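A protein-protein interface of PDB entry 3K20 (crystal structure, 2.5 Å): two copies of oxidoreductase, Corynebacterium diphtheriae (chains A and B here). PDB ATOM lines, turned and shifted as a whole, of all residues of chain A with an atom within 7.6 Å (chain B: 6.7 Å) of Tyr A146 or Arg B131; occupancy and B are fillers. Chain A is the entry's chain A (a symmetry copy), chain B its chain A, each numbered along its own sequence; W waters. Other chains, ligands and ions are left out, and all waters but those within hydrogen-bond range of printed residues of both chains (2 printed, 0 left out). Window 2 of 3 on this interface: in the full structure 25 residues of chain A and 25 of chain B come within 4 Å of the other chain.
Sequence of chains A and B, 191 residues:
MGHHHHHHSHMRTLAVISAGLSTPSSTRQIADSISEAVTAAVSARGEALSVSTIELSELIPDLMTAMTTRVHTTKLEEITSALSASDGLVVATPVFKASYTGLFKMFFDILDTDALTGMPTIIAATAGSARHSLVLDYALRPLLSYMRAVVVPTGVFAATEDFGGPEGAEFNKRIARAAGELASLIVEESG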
ATOM      1  N   THR A 113      19.871  16.473  29.562  1.00  0.00           N
ATOM      2  CA  THR A 113      19.017  15.363  29.187  1.00  0.00           C
ATOM      3  C   THR A 113      17.559  15.741  28.914  1.00  0.00           C
ATOM      4  O   THR A 113      16.970  15.292  27.933  1.00  0.00           O
ATOM      5  CB  THR A 113      19.086  14.262  30.266  1.00  0.00           C
ATOM      6  OG1 THR A 113      20.413  13.713  30.276  1.00  0.00           O
ATOM      7  CG2 THR A 113      18.095  13.150  29.980  1.00  0.00           C
ATOM      8  N   THR A 117      12.495  17.674  26.063  1.00  0.00           N
ATOM      9  CA  THR A 117      11.347  16.828  26.347  1.00  0.00           C
ATOM     10  C   THR A 117      10.041  17.491  25.853  1.00  0.00           C
ATOM     11  O   THR A 117       9.745  18.638  26.202  1.00  0.00           O
ATOM     12  CB  THR A 117      11.238  16.552  27.866  1.00  0.00           C
ATOM     13  OG1 THR A 117      12.484  16.028  28.348  1.00  0.00           O
ATOM     14  CG2 THR A 117      10.127  15.555  28.146  1.00  0.00           C
ATOM     15  N   LEU A 140      18.680  11.646  12.493  1.00  0.00           N
ATOM     16  CA  LEU A 140      18.060  12.733  13.227  1.00  0.00           C
ATOM     17  C   LEU A 140      16.850  12.313  14.035  1.00  0.00           C
ATOM     18  O   LEU A 140      16.656  12.780  15.169  1.00  0.00           O
ATOM     19  CB  LEU A 140      17.669  13.877  12.288  1.00  0.00           C
ATOM     20  CG  LEU A 140      18.836  14.679  11.705  1.00  0.00           C
ATOM     21  CD1 LEU A 140      19.337  14.014  10.428  1.00  0.00           C
ATOM     22  CD2 LEU A 140      18.376  16.088  11.414  1.00  0.00           C
ATOM     23  N   ARG A 141      16.043  11.422  13.470  1.00  0.00           N
ATOM     24  CA  ARG A 141      14.838  10.990  14.163  1.00  0.00           C
ATOM     25  C   ARG A 141      15.192  10.273  15.452  1.00  0.00           C
ATOM     26  O   ARG A 141      14.654  10.582  16.515  1.00  0.00           O
ATOM     27  CB  ARG A 141      13.995  10.089  13.263  1.00  0.00           C
ATOM     28  CG  ARG A 141      12.561   9.948  13.744  1.00  0.00           C
ATOM     29  CD  ARG A 141      11.589  10.039  12.586  1.00  0.00           C
ATOM     30  NE  ARG A 141      10.377  10.707  13.028  1.00  0.00           N
ATOM     31  CZ  ARG A 141       9.694  11.589  12.307  1.00  0.00           C
ATOM     32  NH1 ARG A 141      10.087  11.923  11.081  1.00  0.00           N
ATOM     33  NH2 ARG A 141       8.627  12.158  12.838  1.00  0.00           N
ATOM     34  N   PRO A 142      16.104   9.298  15.379  1.00  0.00           N
ATOM     35  CA  PRO A 142      16.464   8.596  16.608  1.00  0.00           C
ATOM     36  C   PRO A 142      17.016   9.572  17.643  1.00  0.00           C
ATOM     37  O   PRO A 142      16.773   9.410  18.832  1.00  0.00           O
ATOM     38  CB  PRO A 142      17.512   7.593  16.137  1.00  0.00           C
ATOM     39  CG  PRO A 142      17.100   7.322  14.704  1.00  0.00           C
ATOM     40  CD  PRO A 142      16.779   8.705  14.209  1.00  0.00           C
ATOM     41  N   LEU A 143      17.752  10.586  17.183  1.00  0.00           N
ATOM     42  CA  LEU A 143      18.350  11.584  18.075  1.00  0.00           C
ATOM     43  C   LEU A 143      17.323  12.437  18.829  1.00  0.00           C
ATOM     44  O   LEU A 143      17.356  12.502  20.063  1.00  0.00           O
ATOM     45  CB  LEU A 143      19.283  12.510  17.292  1.00  0.00           C
ATOM     46  CG  LEU A 143      19.944  13.625  18.127  1.00  0.00           C
ATOM     47  CD1 LEU A 143      20.905  13.033  19.172  1.00  0.00           C
ATOM     48  CD2 LEU A 143      20.692  14.563  17.197  1.00  0.00           C
ATOM     49  N   LEU A 144      16.429  13.103  18.094  1.00  0.00           N
ATOM     50  CA  LEU A 144      15.404  13.938  18.724  1.00  0.00           C
ATOM     51  C   LEU A 144      14.437  13.067  19.525  1.00  0.00           C
ATOM     52  O   LEU A 144      13.848  13.513  20.517  1.00  0.00           O
ATOM     53  CB  LEU A 144      14.638  14.744  17.668  1.00  0.00           C
ATOM     54  CG  LEU A 144      15.273  16.056  17.176  1.00  0.00           C
ATOM     55  CD1 LEU A 144      15.287  17.093  18.294  1.00  0.00           C
ATOM     56  CD2 LEU A 144      16.686  15.787  16.695  1.00  0.00           C
ATOM     57  N   SER A 145      14.277  11.821  19.090  1.00  0.00           N
ATOM     58  CA  SER A 145      13.405  10.896  19.790  1.00  0.00           C
ATOM     59  C   SER A 145      14.051  10.510  21.110  1.00  0.00           C
ATOM     60  O   SER A 145      13.381  10.440  22.146  1.00  0.00           O
ATOM     61  CB  SER A 145      13.150   9.644  18.949  1.00  0.00           C
ATOM     62  OG  SER A 145      12.220   9.918  17.921  1.00  0.00           O
ATOM     63  N   TYR A 146      15.354  10.264  21.091  1.00  0.00           N
ATOM     64  CA  TYR A 146      16.026   9.902  22.321  1.00  0.00           C
ATOM     65  C   TYR A 146      15.806  11.001  23.359  1.00  0.00           C
ATOM     66  O   TYR A 146      15.761  10.736  24.565  1.00  0.00           O
ATOM     67  CB  TYR A 146      17.516   9.722  22.084  1.00  0.00           C
ATOM     68  CG  TYR A 146      18.285   9.557  23.363  1.00  0.00           C
ATOM     69  CD1 TYR A 146      18.172   8.397  24.119  1.00  0.00           C
ATOM     70  CD2 TYR A 146      19.115  10.569  23.828  1.00  0.00           C
ATOM     71  CE1 TYR A 146      18.872   8.244  25.309  1.00  0.00           C
ATOM     72  CE2 TYR A 146      19.821  10.434  25.012  1.00  0.00           C
ATOM     73  CZ  TYR A 146      19.700   9.269  25.750  1.00  0.00           C
ATOM     74  OH  TYR A 146      20.422   9.126  26.918  1.00  0.00           O
ATOM     75  N   MET A 147      15.670  12.232  22.879  1.00  0.00           N
ATOM     76  CA  MET A 147      15.458  13.365  23.760  1.00  0.00           C
ATOM     77  C   MET A 147      13.989  13.650  23.997  1.00  0.00           C
ATOM     78  O   MET A 147      13.608  14.736  24.429  1.00  0.00           O
ATOM     79  CB  MET A 147      16.169  14.583  23.199  1.00  0.00           C
ATOM     80  CG  MET A 147      17.658  14.364  23.188  1.00  0.00           C
ATOM     81  SD  MET A 147      18.665  15.931  22.839  1.00  0.00           S
ATOM     82  CE  MET A 147      19.632  15.338  21.280  1.00  0.00           C
ATOM     83  N   ARG A 148      13.171  12.649  23.717  1.00  0.00           N
ATOM     84  CA  ARG A 148      11.743  12.752  23.927  1.00  0.00           C
ATOM     85  C   ARG A 148      11.075  13.950  23.249  1.00  0.00           C
ATOM     86  O   ARG A 148      10.031  14.416  23.708  1.00  0.00           O
ATOM     87  CB  ARG A 148      11.447  12.768  25.430  1.00  0.00           C
ATOM     88  CG  ARG A 148      12.075  11.607  26.209  1.00  0.00           C
ATOM     89  CD  ARG A 148      11.758  11.724  27.701  1.00  0.00           C
ATOM     90  NE  ARG A 148      10.313  11.763  27.940  1.00  0.00           N
ATOM     91  CZ  ARG A 148       9.749  12.078  29.103  1.00  0.00           C
ATOM     92  NH1 ARG A 148      10.509  12.384  30.149  1.00  0.00           N
ATOM     93  NH2 ARG A 148       8.423  12.096  29.220  1.00  0.00           N
ATOM     94  N   ALA A 149      11.663  14.468  22.177  1.00  0.00           N
ATOM     95  CA  ALA A 149      11.019  15.571  21.472  1.00  0.00           C
ATOM     96  C   ALA A 149       9.980  14.927  20.559  1.00  0.00           C
ATOM     97  O   ALA A 149      10.131  13.771  20.161  1.00  0.00           O
ATOM     98  CB  ALA A 149      12.026  16.334  20.628  1.00  0.00           C
ATOM     99  N   VAL A 151       8.851  14.713  17.085  1.00  0.00           N
ATOM    100  CA  VAL A 151       9.215  15.022  15.701  1.00  0.00           C
ATOM    101  C   VAL A 151       8.050  14.766  14.758  1.00  0.00           C
ATOM    102  O   VAL A 151       7.583  13.637  14.645  1.00  0.00           O
ATOM    103  CB  VAL A 151      10.389  14.147  15.229  1.00  0.00           C
ATOM    104  CG1 VAL A 151      10.786  14.526  13.807  1.00  0.00           C
ATOM    105  CG2 VAL A 151      11.560  14.290  16.192  1.00  0.00           C
ATOM    106  N   VAL B  95      29.007   6.957  24.374  1.00  0.00           N
ATOM    107  CA  VAL B  95      27.694   7.120  23.773  1.00  0.00           C
ATOM    108  C   VAL B  95      26.989   8.346  24.364  1.00  0.00           C
ATOM    109  O   VAL B  95      26.608   8.358  25.533  1.00  0.00           O
ATOM    110  CB  VAL B  95      26.834   5.858  23.959  1.00  0.00           C
ATOM    111  CG1 VAL B  95      25.487   6.041  23.267  1.00  0.00           C
ATOM    112  CG2 VAL B  95      27.567   4.648  23.378  1.00  0.00           C
ATOM    113  N   PHE B  96      26.852   9.386  23.543  1.00  0.00           N
ATOM    114  CA  PHE B  96      26.188  10.624  23.946  1.00  0.00           C
ATOM    115  C   PHE B  96      24.889  10.707  23.173  1.00  0.00           C
ATOM    116  O   PHE B  96      24.870  10.485  21.967  1.00  0.00           O
ATOM    117  CB  PHE B  96      27.038  11.856  23.595  1.00  0.00           C
ATOM    118  CG  PHE B  96      28.265  12.034  24.451  1.00  0.00           C
ATOM    119  CD1 PHE B  96      28.499  11.213  25.557  1.00  0.00           C
ATOM    120  CD2 PHE B  96      29.173  13.055  24.167  1.00  0.00           C
ATOM    121  CE1 PHE B  96      29.620  11.407  26.372  1.00  0.00           C
ATOM    122  CE2 PHE B  96      30.303  13.261  24.978  1.00  0.00           C
ATOM    123  CZ  PHE B  96      30.524  12.431  26.084  1.00  0.00           C
ATOM    124  N   LYS B  97      23.805  11.036  23.858  1.00  0.00           N
ATOM    125  CA  LYS B  97      22.505  11.135  23.210  1.00  0.00           C
ATOM    126  C   LYS B  97      22.201   9.924  22.323  1.00  0.00           C
ATOM    127  O   LYS B  97      21.800  10.076  21.170  1.00  0.00           O
ATOM    128  CB  LYS B  97      22.430  12.407  22.368  1.00  0.00           C
ATOM    129  CG  LYS B  97      22.819  13.663  23.117  1.00  0.00           C
ATOM    130  CD  LYS B  97      21.842  13.993  24.229  1.00  0.00           C
ATOM    131  CE  LYS B  97      22.398  15.114  25.101  1.00  0.00           C
ATOM    132  NZ  LYS B  97      21.438  15.495  26.165  1.00  0.00           N
ATOM    133  N   ALA B  98      22.411   8.728  22.868  1.00  0.00           N
ATOM    134  CA  ALA B  98      22.134   7.469  22.173  1.00  0.00           C
ATOM    135  C   ALA B  98      22.879   7.237  20.856  1.00  0.00           C
ATOM    136  O   ALA B  98      22.340   6.600  19.945  1.00  0.00           O
ATOM    137  CB  ALA B  98      20.629   7.333  21.936  1.00  0.00           C
ATOM    138  N   SER B  99      24.105   7.743  20.748  1.00  0.00           N
ATOM    139  CA  SER B  99      24.889   7.550  19.532  1.00  0.00           C
ATOM    140  C   SER B  99      26.338   8.005  19.698  1.00  0.00           C
ATOM    141  O   SER B  99      26.769   8.330  20.810  1.00  0.00           O
ATOM    142  CB  SER B  99      24.250   8.295  18.363  1.00  0.00           C
ATOM    143  OG  SER B  99      24.941   8.004  17.155  1.00  0.00           O
ATOM    144  N   GLY B 128      27.460   2.808  30.240  1.00  0.00           N
ATOM    145  CA  GLY B 128      27.150   2.092  31.461  1.00  0.00           C
ATOM    146  C   GLY B 128      26.509   0.765  31.114  1.00  0.00           C
ATOM    147  O   GLY B 128      27.123  -0.282  31.295  1.00  0.00           O
ATOM    148  N   SER B 129      25.280   0.814  30.602  1.00  0.00           N
ATOM    149  CA  SER B 129      24.553  -0.396  30.222  1.00  0.00           C
ATOM    150  C   SER B 129      24.764  -0.761  28.751  1.00  0.00           C
ATOM    151  O   SER B 129      25.502  -0.092  28.023  1.00  0.00           O
ATOM    152  CB  SER B 129      23.050  -0.234  30.483  1.00  0.00           C
ATOM    153  OG  SER B 129      22.421   0.519  29.461  1.00  0.00           O
ATOM    154  N   ALA B 130      24.094  -1.820  28.316  1.00  0.00           N
ATOM    155  CA  ALA B 130      24.218  -2.278  26.940  1.00  0.00           C
ATOM    156  C   ALA B 130      22.988  -1.964  26.074  1.00  0.00           C
ATOM    157  O   ALA B 130      22.898  -2.419  24.931  1.00  0.00           O
ATOM    158  CB  ALA B 130      24.501  -3.782  26.926  1.00  0.00           C
ATOM    159  N   ARG B 131      22.059  -1.172  26.602  1.00  0.00           N
ATOM    160  CA  ARG B 131      20.852  -0.851  25.846  1.00  0.00           C
ATOM    161  C   ARG B 131      21.101  -0.048  24.565  1.00  0.00           C
ATOM    162  O   ARG B 131      20.245  -0.002  23.682  1.00  0.00           O
ATOM    163  CB  ARG B 131      19.827  -0.125  26.739  1.00  0.00           C
ATOM    164  CG  ARG B 131      20.090   1.346  27.057  1.00  0.00           C
ATOM    165  CD  ARG B 131      18.825   1.948  27.700  1.00  0.00           C
ATOM    166  NE  ARG B 131      18.768   3.415  27.653  1.00  0.00           N
ATOM    167  CZ  ARG B 131      19.502   4.227  28.409  1.00  0.00           C
ATOM    168  NH1 ARG B 131      20.364   3.725  29.286  1.00  0.00           N
ATOM    169  NH2 ARG B 131      19.371   5.542  28.291  1.00  0.00           N
ATOM    170  N   HIS B 132      22.271   0.569  24.460  1.00  0.00           N
ATOM    171  CA  HIS B 132      22.614   1.357  23.279  1.00  0.00           C
ATOM    172  C   HIS B 132      23.730   0.693  22.476  1.00  0.00           C
ATOM    173  O   HIS B 132      24.439   1.355  21.716  1.00  0.00           O
ATOM    174  CB  HIS B 132      23.041   2.770  23.699  1.00  0.00           C
ATOM    175  CG  HIS B 132      21.909   3.621  24.181  1.00  0.00           C
ATOM    176  ND1 HIS B 132      22.088   4.695  25.029  1.00  0.00           N
ATOM    177  CD2 HIS B 132      20.577   3.556  23.933  1.00  0.00           C
ATOM    178  CE1 HIS B 132      20.917   5.251  25.284  1.00  0.00           C
ATOM    179  NE2 HIS B 132      19.983   4.579  24.632  1.00  0.00           N
ATOM    180  N   SER B 133      23.887  -0.618  22.636  1.00  0.00           N
ATOM    181  CA  SER B 133      24.941  -1.318  21.916  1.00  0.00           C
ATOM    182  C   SER B 133      24.716  -1.358  20.399  1.00  0.00           C
ATOM    183  O   SER B 133      25.681  -1.484  19.641  1.00  0.00           O
ATOM    184  CB  SER B 133      25.121  -2.741  22.473  1.00  0.00           C
ATOM    185  OG  SER B 133      23.944  -3.509  22.355  1.00  0.00           O
ATOM    186  N   LEU B 134      23.462  -1.234  19.958  1.00  0.00           N
ATOM    187  CA  LEU B 134      23.146  -1.256  18.525  1.00  0.00           C
ATOM    188  C   LEU B 134      23.698  -0.028  17.805  1.00  0.00           C
ATOM    189  O   LEU B 134      23.601   0.097  16.580  1.00  0.00           O
ATOM    190  CB  LEU B 134      21.631  -1.359  18.292  1.00  0.00           C
ATOM    191  CG  LEU B 134      21.021  -2.768  18.266  1.00  0.00           C
ATOM    192  CD1 LEU B 134      19.495  -2.680  18.055  1.00  0.00           C
ATOM    193  CD2 LEU B 134      21.686  -3.593  17.159  1.00  0.00           C
ATOM    194  N   VAL B 135      24.282   0.881  18.570  1.00  0.00           N
ATOM    195  CA  VAL B 135      24.877   2.067  17.990  1.00  0.00           C
ATOM    196  C   VAL B 135      26.027   1.619  17.067  1.00  0.00           C
ATOM    197  O   VAL B 135      26.381   2.313  16.114  1.00  0.00           O
ATOM    198  CB  VAL B 135      25.422   2.988  19.097  1.00  0.00           C
ATOM    199  CG1 VAL B 135      26.622   2.335  19.764  1.00  0.00           C
ATOM    200  CG2 VAL B 135      25.783   4.349  18.524  1.00  0.00           C
ATOM    201  N   PHE B 157      31.350  -3.626  22.109  1.00  0.00           N
ATOM    202  CA  PHE B 157      30.587  -2.685  22.921  1.00  0.00           C
ATOM    203  C   PHE B 157      30.789  -2.955  24.405  1.00  0.00           C
ATOM    204  O   PHE B 157      30.239  -3.911  24.947  1.00  0.00           O
ATOM    205  CB  PHE B 157      29.089  -2.757  22.625  1.00  0.00           C
ATOM    206  CG  PHE B 157      28.328  -1.581  23.163  1.00  0.00           C
ATOM    207  CD1 PHE B 157      28.263  -0.389  22.434  1.00  0.00           C
ATOM    208  CD2 PHE B 157      27.766  -1.618  24.437  1.00  0.00           C
ATOM    209  CE1 PHE B 157      27.655   0.749  22.964  1.00  0.00           C
ATOM    210  CE2 PHE B 157      27.156  -0.486  24.981  1.00  0.00           C
ATOM    211  CZ  PHE B 157      27.103   0.705  24.240  1.00  0.00           C
ATOM    212  N   ALA B 159      30.019  -2.474  28.084  1.00  0.00           N
ATOM    213  CA  ALA B 159      29.008  -1.993  29.013  1.00  0.00           C
ATOM    214  C   ALA B 159      29.690  -2.072  30.382  1.00  0.00           C
ATOM    215  O   ALA B 159      29.819  -3.154  30.957  1.00  0.00           O
ATOM    216  CB  ALA B 159      27.781  -2.880  28.968  1.00  0.00           C
HETATM  217  O   HOH W   1      20.582   9.353  18.772  1.00  0.00           O
HETATM  218  O   HOH W   2      23.107   8.116  25.539  1.00  0.00           O
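The side-chain hydroxyl of Ser B129 is in hydrogen-bond range of the backbone NH of Arg B131.
The guanidinium group (NE) of Arg B131 is in hydrogen-bond range of a ring nitrogen (NE2) of His B132 (3.5 Å).
No position is printed for both chains.
Printed residues of chain A that touch a printed residue of chain B: Thr A113, Leu A143, Tyr A146 and Met A147.
Hydrophobic or aromatic side chains of chain A that line the printed part of chain B: Leu A143, Tyr A146 and Met A147.
Of the 15 printed residues of chain B, 4 touch a printed residue of chain A.
Of the printed residues of chain B, Thr A113 touches Lys B97.
Tyr A146 touches just these residues of chain B: Lys B97 (3.3 Å), Ala B98 (3.5 Å), Arg B131 (3.98 Å) and His B132 (3.6 Å).
Printed residues of chain A within 4 Å of Lys B97: Thr A113, Leu A143, Tyr A146 and Met A147.
Of chain A, only Tyr A146 (3.98 Å) comes within 4 Å of Arg B131.
Of the printed residues of chain A, His B132 touches Tyr A146.
Phe B157 touches none of the printed residues of chain A.
The nearest residue of chain B that does not touch Tyr A146 is Phe B96 (5.4 Å).
NZ of Lys B97 touches N of Thr A113, at 3.9 Å.
Leu A143 touches Lys B97 (CD1 to CB, 3.6 Å).
CE2 of Tyr A146 touches CA of Lys B97, at 3.3 Å.
Ala B98 touches Tyr A146.
Arg B131 touches Tyr A146 (NH2 to OH, 3.98 Å).
CE1 of His B132 touches CE1 of Tyr A146, 3.6 Å away.
Met A147 touches Lys B97 (CE to CD, 3.9 Å).
Water W1 lies within hydrogen-bond range of O of Lys B97 (2.8 Å), O of Ala B98 (3.5 Å) and N of Leu A143 (3.5 Å).
Water W2 lies within hydrogen-bond range of N of Ala B98, OH of Tyr A146 and N of Lys B97.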
